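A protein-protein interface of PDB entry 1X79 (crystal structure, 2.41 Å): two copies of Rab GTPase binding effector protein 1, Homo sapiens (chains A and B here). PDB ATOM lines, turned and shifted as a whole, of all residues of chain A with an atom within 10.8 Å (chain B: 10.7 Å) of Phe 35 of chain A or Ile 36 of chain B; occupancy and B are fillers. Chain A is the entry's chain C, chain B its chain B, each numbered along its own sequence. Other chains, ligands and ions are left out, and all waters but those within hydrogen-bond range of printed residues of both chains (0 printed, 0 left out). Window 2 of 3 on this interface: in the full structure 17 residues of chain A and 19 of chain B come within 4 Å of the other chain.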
ATOM      1  N   LYS A  27       7.913  22.614 -11.770  1.00  0.00           N
ATOM      2  CA  LYS A  27       7.486  21.279 -11.417  1.00  0.00           C
ATOM      3  C   LYS A  27       6.982  21.335  -9.980  1.00  0.00           C
ATOM      4  O   LYS A  27       5.907  20.848  -9.690  1.00  0.00           O
ATOM      5  CB  LYS A  27       8.669  20.324 -11.530  1.00  0.00           C
ATOM      6  CG  LYS A  27       8.330  18.863 -11.434  1.00  0.00           C
ATOM      7  CD  LYS A  27       9.603  18.009 -11.264  1.00  0.00           C
ATOM      8  CE  LYS A  27       9.312  16.506 -11.458  1.00  0.00           C
ATOM      9  NZ  LYS A  27      10.510  15.599 -11.368  1.00  0.00           N
ATOM     10  N   ASP A  28       7.756  21.942  -9.086  1.00  0.00           N
ATOM     11  CA  ASP A  28       7.372  22.085  -7.688  1.00  0.00           C
ATOM     12  C   ASP A  28       6.031  22.788  -7.487  1.00  0.00           C
ATOM     13  O   ASP A  28       5.231  22.373  -6.658  1.00  0.00           O
ATOM     14  CB  ASP A  28       8.435  22.851  -6.914  1.00  0.00           C
ATOM     15  CG  ASP A  28       9.717  22.063  -6.745  1.00  0.00           C
ATOM     16  OD1 ASP A  28       9.765  20.877  -7.164  1.00  0.00           O
ATOM     17  OD2 ASP A  28      10.679  22.642  -6.182  1.00  0.00           O
ATOM     18  N   LYS A  29       5.788  23.860  -8.218  1.00  0.00           N
ATOM     19  CA  LYS A  29       4.506  24.516  -8.103  1.00  0.00           C
ATOM     20  C   LYS A  29       3.387  23.608  -8.576  1.00  0.00           C
ATOM     21  O   LYS A  29       2.357  23.504  -7.919  1.00  0.00           O
ATOM     22  CB  LYS A  29       4.502  25.819  -8.888  1.00  0.00           C
ATOM     23  CG  LYS A  29       3.130  26.322  -9.201  1.00  0.00           C
ATOM     24  CD  LYS A  29       3.163  27.702  -9.797  1.00  0.00           C
ATOM     25  CE  LYS A  29       1.949  27.943 -10.658  1.00  0.00           C
ATOM     26  NZ  LYS A  29       1.948  29.330 -11.198  1.00  0.00           N
ATOM     27  N   GLN A  30       3.585  22.937  -9.706  1.00  0.00           N
ATOM     28  CA  GLN A  30       2.592  21.999 -10.234  1.00  0.00           C
ATOM     29  C   GLN A  30       2.235  20.912  -9.210  1.00  0.00           C
ATOM     30  O   GLN A  30       1.063  20.553  -9.055  1.00  0.00           O
ATOM     31  CB  GLN A  30       3.120  21.323 -11.493  1.00  0.00           C
ATOM     32  CG  GLN A  30       2.183  20.276 -12.064  1.00  0.00           C
ATOM     33  CD  GLN A  30       1.029  20.901 -12.813  1.00  0.00           C
ATOM     34  OE1 GLN A  30       1.110  21.120 -14.027  1.00  0.00           O
ATOM     35  NE2 GLN A  30      -0.049  21.214 -12.094  1.00  0.00           N
ATOM     36  N   GLU A  31       3.248  20.394  -8.525  1.00  0.00           N
ATOM     37  CA  GLU A  31       3.035  19.398  -7.493  1.00  0.00           C
ATOM     38  C   GLU A  31       2.146  19.902  -6.341  1.00  0.00           C
ATOM     39  O   GLU A  31       1.208  19.224  -5.920  1.00  0.00           O
ATOM     40  CB  GLU A  31       4.385  18.935  -6.952  1.00  0.00           C
ATOM     41  CG  GLU A  31       4.787  17.568  -7.465  1.00  0.00           C
ATOM     42  CD  GLU A  31       6.296  17.396  -7.652  1.00  0.00           C
ATOM     43  OE1 GLU A  31       7.082  17.730  -6.726  1.00  0.00           O
ATOM     44  OE2 GLU A  31       6.689  16.907  -8.737  1.00  0.00           O
ATOM     45  N   LEU A  32       2.439  21.088  -5.833  1.00  0.00           N
ATOM     46  CA  LEU A  32       1.628  21.671  -4.792  1.00  0.00           C
ATOM     47  C   LEU A  32       0.221  21.872  -5.317  1.00  0.00           C
ATOM     48  O   LEU A  32      -0.739  21.662  -4.596  1.00  0.00           O
ATOM     49  CB  LEU A  32       2.192  23.026  -4.344  1.00  0.00           C
ATOM     50  CG  LEU A  32       3.578  22.976  -3.719  1.00  0.00           C
ATOM     51  CD1 LEU A  32       4.057  24.380  -3.505  1.00  0.00           C
ATOM     52  CD2 LEU A  32       3.552  22.239  -2.416  1.00  0.00           C
ATOM     53  N   GLU A  33       0.086  22.299  -6.560  1.00  0.00           N
ATOM     54  CA  GLU A  33      -1.247  22.604  -7.041  1.00  0.00           C
ATOM     55  C   GLU A  33      -2.057  21.330  -7.087  1.00  0.00           C
ATOM     56  O   GLU A  33      -3.248  21.341  -6.817  1.00  0.00           O
ATOM     57  CB  GLU A  33      -1.200  23.246  -8.423  1.00  0.00           C
ATOM     58  CG  GLU A  33      -0.725  24.677  -8.397  1.00  0.00           C
ATOM     59  CD  GLU A  33      -0.644  25.268  -9.779  1.00  0.00           C
ATOM     60  OE1 GLU A  33      -0.249  24.503 -10.690  1.00  0.00           O
ATOM     61  OE2 GLU A  33      -0.954  26.480  -9.954  1.00  0.00           O
ATOM     62  N   ASP A  34      -1.395  20.229  -7.419  1.00  0.00           N
ATOM     63  CA  ASP A  34      -2.067  18.959  -7.534  1.00  0.00           C
ATOM     64  C   ASP A  34      -2.491  18.537  -6.168  1.00  0.00           C
ATOM     65  O   ASP A  34      -3.633  18.137  -5.950  1.00  0.00           O
ATOM     66  CB  ASP A  34      -1.137  17.898  -8.114  1.00  0.00           C
ATOM     67  CG  ASP A  34      -0.875  18.091  -9.607  1.00  0.00           C
ATOM     68  OD1 ASP A  34      -1.682  18.792 -10.290  1.00  0.00           O
ATOM     69  OD2 ASP A  34       0.139  17.518 -10.085  1.00  0.00           O
ATOM     70  N   PHE A  35      -1.551  18.615  -5.245  1.00  0.00           N
ATOM     71  CA  PHE A  35      -1.823  18.285  -3.864  1.00  0.00           C
ATOM     72  C   PHE A  35      -3.057  19.023  -3.372  1.00  0.00           C
ATOM     73  O   PHE A  35      -4.000  18.424  -2.880  1.00  0.00           O
ATOM     74  CB  PHE A  35      -0.652  18.685  -3.014  1.00  0.00           C
ATOM     75  CG  PHE A  35      -0.852  18.430  -1.578  1.00  0.00           C
ATOM     76  CD1 PHE A  35      -0.732  17.149  -1.068  1.00  0.00           C
ATOM     77  CD2 PHE A  35      -1.145  19.472  -0.718  1.00  0.00           C
ATOM     78  CE1 PHE A  35      -0.899  16.906   0.295  1.00  0.00           C
ATOM     79  CE2 PHE A  35      -1.317  19.237   0.654  1.00  0.00           C
ATOM     80  CZ  PHE A  35      -1.192  17.952   1.157  1.00  0.00           C
ATOM     81  N   ILE A  36      -3.045  20.336  -3.505  1.00  0.00           N
ATOM     82  CA  ILE A  36      -4.182  21.119  -3.097  1.00  0.00           C
ATOM     83  C   ILE A  36      -5.457  20.545  -3.681  1.00  0.00           C
ATOM     84  O   ILE A  36      -6.493  20.583  -3.043  1.00  0.00           O
ATOM     85  CB  ILE A  36      -4.015  22.583  -3.519  1.00  0.00           C
ATOM     86  CG1 ILE A  36      -2.908  23.215  -2.679  1.00  0.00           C
ATOM     87  CG2 ILE A  36      -5.319  23.363  -3.342  1.00  0.00           C
ATOM     88  CD1 ILE A  36      -2.629  24.670  -3.043  1.00  0.00           C
ATOM     89  N   LYS A  37      -5.383  19.989  -4.883  1.00  0.00           N
ATOM     90  CA  LYS A  37      -6.588  19.535  -5.573  1.00  0.00           C
ATOM     91  C   LYS A  37      -7.035  18.182  -5.047  1.00  0.00           C
ATOM     92  O   LYS A  37      -8.210  17.973  -4.775  1.00  0.00           O
ATOM     93  CB  LYS A  37      -6.332  19.445  -7.072  1.00  0.00           C
ATOM     94  CG  LYS A  37      -7.577  19.166  -7.890  1.00  0.00           C
ATOM     95  CD  LYS A  37      -7.438  19.642  -9.338  1.00  0.00           C
ATOM     96  CE  LYS A  37      -8.572  19.111 -10.215  1.00  0.00           C
ATOM     97  NZ  LYS A  37      -8.570  17.613 -10.182  1.00  0.00           N
ATOM     98  N   GLN A  38      -6.089  17.268  -4.902  1.00  0.00           N
ATOM     99  CA  GLN A  38      -6.395  15.952  -4.404  1.00  0.00           C
ATOM    100  C   GLN A  38      -6.984  16.073  -3.031  1.00  0.00           C
ATOM    101  O   GLN A  38      -8.001  15.482  -2.726  1.00  0.00           O
ATOM    102  CB  GLN A  38      -5.138  15.118  -4.303  1.00  0.00           C
ATOM    103  CG  GLN A  38      -5.418  13.665  -4.081  1.00  0.00           C
ATOM    104  CD  GLN A  38      -6.391  13.139  -5.100  1.00  0.00           C
ATOM    105  OE1 GLN A  38      -6.306  13.450  -6.294  1.00  0.00           O
ATOM    106  NE2 GLN A  38      -7.328  12.335  -4.637  1.00  0.00           N
ATOM    107  N   SER A  39      -6.325  16.838  -2.181  1.00  0.00           N
ATOM    108  CA  SER A  39      -6.681  16.806  -0.787  1.00  0.00           C
ATOM    109  C   SER A  39      -8.010  17.530  -0.712  1.00  0.00           C
ATOM    110  O   SER A  39      -8.919  17.122  -0.003  1.00  0.00           O
ATOM    111  CB  SER A  39      -5.617  17.514   0.065  1.00  0.00           C
ATOM    112  OG  SER A  39      -5.878  18.895   0.094  1.00  0.00           O
ATOM    113  N   SER A  40      -8.144  18.596  -1.474  1.00  0.00           N
ATOM    114  CA  SER A  40      -9.401  19.297  -1.481  1.00  0.00           C
ATOM    115  C   SER A  40     -10.586  18.430  -1.921  1.00  0.00           C
ATOM    116  O   SER A  40     -11.694  18.581  -1.422  1.00  0.00           O
ATOM    117  CB  SER A  40      -9.298  20.521  -2.374  1.00  0.00           C
ATOM    118  OG  SER A  40     -10.524  21.216  -2.379  1.00  0.00           O
ATOM    119  N   GLU A  41     -10.372  17.524  -2.860  1.00  0.00           N
ATOM    120  CA  GLU A  41     -11.483  16.706  -3.317  1.00  0.00           C
ATOM    121  C   GLU A  41     -11.785  15.645  -2.280  1.00  0.00           C
ATOM    122  O   GLU A  41     -12.941  15.321  -2.040  1.00  0.00           O
ATOM    123  CB  GLU A  41     -11.166  16.033  -4.660  1.00  0.00           C
ATOM    124  CG  GLU A  41     -10.862  17.002  -5.792  1.00  0.00           C
ATOM    125  CD  GLU A  41     -10.530  16.296  -7.105  1.00  0.00           C
ATOM    126  OE1 GLU A  41     -10.067  15.130  -7.063  1.00  0.00           O
ATOM    127  OE2 GLU A  41     -10.720  16.921  -8.176  1.00  0.00           O
ATOM    128  N   ASP A  42     -10.738  15.091  -1.685  1.00  0.00           N
ATOM    129  CA  ASP A  42     -10.916  14.137  -0.627  1.00  0.00           C
ATOM    130  C   ASP A  42     -11.762  14.722   0.485  1.00  0.00           C
ATOM    131  O   ASP A  42     -12.557  14.015   1.090  1.00  0.00           O
ATOM    132  CB  ASP A  42      -9.579  13.713  -0.057  1.00  0.00           C
ATOM    133  CG  ASP A  42      -8.763  12.939  -1.044  1.00  0.00           C
ATOM    134  OD1 ASP A  42      -9.351  12.428  -2.032  1.00  0.00           O
ATOM    135  OD2 ASP A  42      -7.538  12.827  -0.828  1.00  0.00           O
ATOM    136  N   SER A  43     -11.591  16.010   0.756  1.00  0.00           N
ATOM    137  CA  SER A  43     -12.324  16.646   1.829  1.00  0.00           C
ATOM    138  C   SER A  43     -13.803  16.693   1.514  1.00  0.00           C
ATOM    139  O   SER A  43     -14.623  16.349   2.365  1.00  0.00           O
ATOM    140  CB  SER A  43     -11.803  18.057   2.086  1.00  0.00           C
ATOM    141  OG  SER A  43     -10.571  18.003   2.768  1.00  0.00           O
ATOM    142  N   SER A  44     -14.152  17.112   0.304  1.00  0.00           N
ATOM    143  CA  SER A  44     -15.532  16.996  -0.121  1.00  0.00           C
ATOM    144  C   SER A  44     -16.130  15.618   0.175  1.00  0.00           C
ATOM    145  O   SER A  44     -17.098  15.512   0.921  1.00  0.00           O
ATOM    146  CB  SER A  44     -15.645  17.294  -1.597  1.00  0.00           C
ATOM    147  OG  SER A  44     -15.538  18.684  -1.759  1.00  0.00           O
ATOM    148  N   ASP B  28       4.744  32.467  -6.557  1.00  0.00           N
ATOM    149  CA  ASP B  28       3.579  31.583  -6.565  1.00  0.00           C
ATOM    150  C   ASP B  28       3.793  30.321  -5.711  1.00  0.00           C
ATOM    151  O   ASP B  28       2.959  29.965  -4.907  1.00  0.00           O
ATOM    152  CB  ASP B  28       3.227  31.160  -7.998  1.00  0.00           C
ATOM    153  CG  ASP B  28       2.753  32.315  -8.860  1.00  0.00           C
ATOM    154  OD1 ASP B  28       2.520  33.414  -8.322  1.00  0.00           O
ATOM    155  OD2 ASP B  28       2.619  32.114 -10.089  1.00  0.00           O
ATOM    156  N   LYS B  29       4.904  29.634  -5.895  1.00  0.00           N
ATOM    157  CA  LYS B  29       5.147  28.437  -5.127  1.00  0.00           C
ATOM    158  C   LYS B  29       4.983  28.761  -3.652  1.00  0.00           C
ATOM    159  O   LYS B  29       4.445  27.962  -2.905  1.00  0.00           O
ATOM    160  CB  LYS B  29       6.555  27.944  -5.379  1.00  0.00           C
ATOM    161  CG  LYS B  29       6.861  26.600  -4.796  1.00  0.00           C
ATOM    162  CD  LYS B  29       8.343  26.390  -4.808  1.00  0.00           C
ATOM    163  CE  LYS B  29       8.767  25.103  -4.161  1.00  0.00           C
ATOM    164  NZ  LYS B  29      10.243  25.042  -4.252  1.00  0.00           N
ATOM    165  N   GLN B  30       5.444  29.931  -3.227  1.00  0.00           N
ATOM    166  CA  GLN B  30       5.433  30.263  -1.809  1.00  0.00           C
ATOM    167  C   GLN B  30       3.998  30.500  -1.345  1.00  0.00           C
ATOM    168  O   GLN B  30       3.555  29.975  -0.312  1.00  0.00           O
ATOM    169  CB  GLN B  30       6.266  31.519  -1.541  1.00  0.00           C
ATOM    170  CG  GLN B  30       6.291  31.943  -0.068  1.00  0.00           C
ATOM    171  CD  GLN B  30       7.028  30.937   0.815  1.00  0.00           C
ATOM    172  OE1 GLN B  30       8.247  30.726   0.667  1.00  0.00           O
ATOM    173  NE2 GLN B  30       6.290  30.300   1.738  1.00  0.00           N
ATOM    174  N   GLU B  31       3.264  31.287  -2.114  1.00  0.00           N
ATOM    175  CA  GLU B  31       1.868  31.465  -1.804  1.00  0.00           C
ATOM    176  C   GLU B  31       1.159  30.130  -1.611  1.00  0.00           C
ATOM    177  O   GLU B  31       0.437  29.961  -0.640  1.00  0.00           O
ATOM    178  CB  GLU B  31       1.186  32.308  -2.873  1.00  0.00           C
ATOM    179  CG  GLU B  31       1.619  33.773  -2.804  1.00  0.00           C
ATOM    180  CD  GLU B  31       0.794  34.679  -3.719  1.00  0.00           C
ATOM    181  OE1 GLU B  31      -0.403  34.357  -3.957  1.00  0.00           O
ATOM    182  OE2 GLU B  31       1.327  35.717  -4.183  1.00  0.00           O
ATOM    183  N   LEU B  32       1.375  29.174  -2.501  1.00  0.00           N
ATOM    184  CA  LEU B  32       0.748  27.873  -2.346  1.00  0.00           C
ATOM    185  C   LEU B  32       1.166  27.226  -1.041  1.00  0.00           C
ATOM    186  O   LEU B  32       0.314  26.774  -0.282  1.00  0.00           O
ATOM    187  CB  LEU B  32       1.096  26.954  -3.513  1.00  0.00           C
ATOM    188  CG  LEU B  32       0.442  27.450  -4.795  1.00  0.00           C
ATOM    189  CD1 LEU B  32       0.992  26.710  -5.957  1.00  0.00           C
ATOM    190  CD2 LEU B  32      -1.043  27.264  -4.726  1.00  0.00           C
ATOM    191  N   GLU B  33       2.463  27.198  -0.763  1.00  0.00           N
ATOM    192  CA  GLU B  33       2.918  26.647   0.498  1.00  0.00           C
ATOM    193  C   GLU B  33       2.311  27.377   1.691  1.00  0.00           C
ATOM    194  O   GLU B  33       2.065  26.771   2.725  1.00  0.00           O
ATOM    195  CB  GLU B  33       4.426  26.710   0.610  1.00  0.00           C
ATOM    196  CG  GLU B  33       5.129  25.995  -0.486  1.00  0.00           C
ATOM    197  CD  GLU B  33       6.617  25.985  -0.268  1.00  0.00           C
ATOM    198  OE1 GLU B  33       7.124  27.010   0.235  1.00  0.00           O
ATOM    199  OE2 GLU B  33       7.275  24.969  -0.599  1.00  0.00           O
ATOM    200  N   ASP B  34       2.076  28.675   1.542  1.00  0.00           N
ATOM    201  CA  ASP B  34       1.447  29.449   2.595  1.00  0.00           C
ATOM    202  C   ASP B  34      -0.002  29.026   2.764  1.00  0.00           C
ATOM    203  O   ASP B  34      -0.450  28.710   3.859  1.00  0.00           O
ATOM    204  CB  ASP B  34       1.518  30.948   2.287  1.00  0.00           C
ATOM    205  CG  ASP B  34       2.913  31.532   2.519  1.00  0.00           C
ATOM    206  OD1 ASP B  34       3.760  30.851   3.157  1.00  0.00           O
ATOM    207  OD2 ASP B  34       3.156  32.679   2.069  1.00  0.00           O
ATOM    208  N   PHE B  35      -0.738  29.006   1.674  1.00  0.00           N
ATOM    209  CA  PHE B  35      -2.137  28.652   1.749  1.00  0.00           C
ATOM    210  C   PHE B  35      -2.340  27.222   2.195  1.00  0.00           C
ATOM    211  O   PHE B  35      -3.324  26.927   2.855  1.00  0.00           O
ATOM    212  CB  PHE B  35      -2.777  28.878   0.407  1.00  0.00           C
ATOM    213  CG  PHE B  35      -4.023  28.101   0.182  1.00  0.00           C
ATOM    214  CD1 PHE B  35      -3.978  26.723   0.007  1.00  0.00           C
ATOM    215  CD2 PHE B  35      -5.243  28.760   0.056  1.00  0.00           C
ATOM    216  CE1 PHE B  35      -5.109  26.028  -0.293  1.00  0.00           C
ATOM    217  CE2 PHE B  35      -6.387  28.060  -0.247  1.00  0.00           C
ATOM    218  CZ  PHE B  35      -6.316  26.691  -0.422  1.00  0.00           C
ATOM    219  N   ILE B  36      -1.432  26.324   1.849  1.00  0.00           N
ATOM    220  CA  ILE B  36      -1.536  24.987   2.401  1.00  0.00           C
ATOM    221  C   ILE B  36      -1.366  25.029   3.920  1.00  0.00           C
ATOM    222  O   ILE B  36      -2.204  24.512   4.658  1.00  0.00           O
ATOM    223  CB  ILE B  36      -0.500  24.039   1.799  1.00  0.00           C
ATOM    224  CG1 ILE B  36      -0.830  23.787   0.327  1.00  0.00           C
ATOM    225  CG2 ILE B  36      -0.501  22.729   2.546  1.00  0.00           C
ATOM    226  CD1 ILE B  36       0.138  22.821  -0.394  1.00  0.00           C
ATOM    227  N   LYS B  37      -0.293  25.655   4.393  1.00  0.00           N
ATOM    228  CA  LYS B  37      -0.014  25.719   5.823  1.00  0.00           C
ATOM    229  C   LYS B  37      -1.187  26.336   6.580  1.00  0.00           C
ATOM    230  O   LYS B  37      -1.665  25.773   7.569  1.00  0.00           O
ATOM    231  CB  LYS B  37       1.249  26.545   6.065  1.00  0.00           C
ATOM    232  CG  LYS B  37       1.766  26.556   7.491  1.00  0.00           C
ATOM    233  CD  LYS B  37       3.177  27.123   7.546  1.00  0.00           C
ATOM    234  CE  LYS B  37       3.505  27.661   8.946  1.00  0.00           C
ATOM    235  NZ  LYS B  37       2.642  28.838   9.314  1.00  0.00           N
ATOM    236  N   GLN B  38      -1.649  27.495   6.119  1.00  0.00           N
ATOM    237  CA  GLN B  38      -2.762  28.141   6.780  1.00  0.00           C
ATOM    238  C   GLN B  38      -3.901  27.170   6.858  1.00  0.00           C
ATOM    239  O   GLN B  38      -4.297  26.765   7.932  1.00  0.00           O
ATOM    240  CB  GLN B  38      -3.241  29.372   6.029  1.00  0.00           C
ATOM    241  CG  GLN B  38      -4.265  30.182   6.819  1.00  0.00           C
ATOM    242  CD  GLN B  38      -3.727  30.626   8.185  1.00  0.00           C
ATOM    243  OE1 GLN B  38      -2.694  31.298   8.272  1.00  0.00           O
ATOM    244  NE2 GLN B  38      -4.423  30.245   9.253  1.00  0.00           N
ATOM    245  N   SER B  39      -4.421  26.788   5.704  1.00  0.00           N
ATOM    246  CA  SER B  39      -5.660  26.033   5.658  1.00  0.00           C
ATOM    247  C   SER B  39      -5.531  24.690   6.412  1.00  0.00           C
ATOM    248  O   SER B  39      -6.463  24.227   7.051  1.00  0.00           O
ATOM    249  CB  SER B  39      -6.047  25.805   4.200  1.00  0.00           C
ATOM    250  OG  SER B  39      -5.590  24.542   3.788  1.00  0.00           O
ATOM    251  N   SER B  40      -4.366  24.077   6.351  1.00  0.00           N
ATOM    252  CA  SER B  40      -4.089  22.927   7.173  1.00  0.00           C
ATOM    253  C   SER B  40      -4.332  23.232   8.660  1.00  0.00           C
ATOM    254  O   SER B  40      -4.991  22.471   9.375  1.00  0.00           O
ATOM    255  CB  SER B  40      -2.643  22.506   6.952  1.00  0.00           C
ATOM    256  OG  SER B  40      -2.269  21.477   7.844  1.00  0.00           O
ATOM    257  N   GLU B  41      -3.790  24.348   9.130  1.00  0.00           N
ATOM    258  CA  GLU B  41      -3.928  24.731  10.531  1.00  0.00           C
ATOM    259  C   GLU B  41      -5.359  25.025  10.924  1.00  0.00           C
ATOM    260  O   GLU B  41      -5.811  24.625  12.000  1.00  0.00           O
ATOM    261  CB  GLU B  41      -3.080  25.960  10.825  1.00  0.00           C
ATOM    262  CG  GLU B  41      -1.638  25.616  11.095  1.00  0.00           C
ATOM    263  CD  GLU B  41      -0.775  26.837  11.100  1.00  0.00           C
ATOM    264  OE1 GLU B  41      -1.343  27.947  11.249  1.00  0.00           O
ATOM    265  OE2 GLU B  41       0.459  26.678  10.959  1.00  0.00           O
ATOM    266  N   ASP B  42      -6.063  25.749  10.064  1.00  0.00           N
ATOM    267  CA  ASP B  42      -7.455  25.985  10.306  1.00  0.00           C
ATOM    268  C   ASP B  42      -8.132  24.656  10.515  1.00  0.00           C
ATOM    269  O   ASP B  42      -8.488  24.326  11.634  1.00  0.00           O
ATOM    270  CB  ASP B  42      -8.081  26.715   9.139  1.00  0.00           C
ATOM    271  CG  ASP B  42      -7.599  28.131   9.038  1.00  0.00           C
ATOM    272  OD1 ASP B  42      -6.945  28.597  10.007  1.00  0.00           O
ATOM    273  OD2 ASP B  42      -7.879  28.781   8.007  1.00  0.00           O
ATOM    274  N   SER B  43      -8.289  23.872   9.458  1.00  0.00           N
ATOM    275  CA  SER B  43      -9.158  22.711   9.531  1.00  0.00           C
ATOM    276  C   SER B  43      -8.827  21.866  10.771  1.00  0.00           C
ATOM    277  O   SER B  43      -9.711  21.296  11.409  1.00  0.00           O
ATOM    278  CB  SER B  43      -9.000  21.871   8.276  1.00  0.00           C
ATOM    279  OG  SER B  43      -7.849  21.074   8.408  1.00  0.00           O
ATOM    280  N   SER B  44      -7.551  21.793  11.123  1.00  0.00           N
ATOM    281  CA  SER B  44      -7.170  21.130  12.358  1.00  0.00           C
ATOM    282  C   SER B  44      -7.939  21.670  13.576  1.00  0.00           C
ATOM    283  O   SER B  44      -8.430  20.902  14.397  1.00  0.00           O
ATOM    284  CB  SER B  44      -5.668  21.274  12.584  1.00  0.00           C
ATOM    285  OG  SER B  44      -5.347  21.128  13.956  1.00  0.00           O
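The side-chain amino group (NZ) of Lys 29 of chain A lies within salt-bridge range of the side-chain carboxylate (OD2) of Asp 28 of chain B, at 3.1 Å. NZ of Lys 29 of chain B is in salt-bridge range of OD2 of Asp 28 of chain A (3.1 Å).
O of Phe 35 of chain B lies close to OG of Ser 39 of chain B. The side-chain hydroxyl of Ser 39 of chain B is in hydrogen-bond range of the backbone carbonyl oxygen of Ile 36 of chain B (3.5 Å).
Among the printed residues, pairs that only touch across the chains: Lys 29 of chain A with Leu 32 of chain B, Leu 32 of chain A with Lys 29 of chain B, Leu 32 of chain A with Leu 32 of chain B, Leu 32 of chain A with Glu 33 of chain B, Glu 33 of chain A with Leu 32 of chain B, Phe 35 of chain A with Ile 36 of chain B, Ile 36 of chain A with Leu 32 of chain B, Ile 36 of chain A with Phe 35 of chain B and Ile 36 of chain A with Ile 36 of chain B.
Printed residues of chain B within 4 Å of Asp 28 of chain A: Lys 29 (3.1 Å). Printed residues of chain B within 4 Å of Lys 29 of chain A: Asp 28 (3.1 Å) and Leu 32 (3.9 Å). No residue of chain B comes within 4 Å of Asp 34 of chain A. Of chain B, only Ile 36 comes within 4 Å of Phe 35 of chain A. Of chain B, only Leu 32, Phe 35 and Ile 36 come within 4 Å of Ile 36 of chain A. Asp 42 of chain A touches none of the printed residues of chain B. Printed residues of chain A within 4 Å of Asp 28 of chain B: Lys 29 (3.1 Å). Of the printed residues of chain A, Leu 32 of chain B touches Lys 29 (3.9 Å), Leu 32 (3.9 Å), Glu 33 (3.6 Å) and Ile 36 (3.5 Å). Of chain A, only Ile 36 comes within 4 Å of Phe 35 of chain B. Printed residues of chain A within 4 Å of Ile 36 of chain B: Phe 35 and Ile 36. No residue of chain A comes within 4 Å of Ser 40 of chain B. The nearest printed residue of chain A that does not touch Ile 36 of chain B is Leu 32 of chain A (4.01 Å). The nearest printed residue of chain A that does not touch Lys 29 of chain B is Lys 29 of chain A (4.5 Å).
Printed residues of chain B that touch a printed residue of chain A: Asp 28, Lys 29, Leu 32, Glu 33, Phe 35 and Ile 36. Hydrophobic or aromatic side chains of chain B that line the printed part of chain A: Leu 32, Phe 35 and Ile 36. Printed residues of chain A that touch a printed residue of chain B: Asp 28, Lys 29, Leu 32, Glu 33, Phe 35 and Ile 36.
Asp 28 of chain A touches Lys 29 of chain B, and with the chains exchanged Lys 29 of chain A touches Asp 28 of chain B. Leu 32 of chain A touches its own counterpart, Leu 32 of chain B. Ile 36 of chain A touches Leu 32 of chain B, but with the chains exchanged Leu 32 of chain A does not touch Ile 36 of chain B (4.01 Å). Ile 36 of chain B touches its own counterpart, Ile 36 of chain A. 17 positions are printed for both chains. Of the 11 pairs that touch across the chains among the printed residues, 10 have their exchanged pair printed and touching as well.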
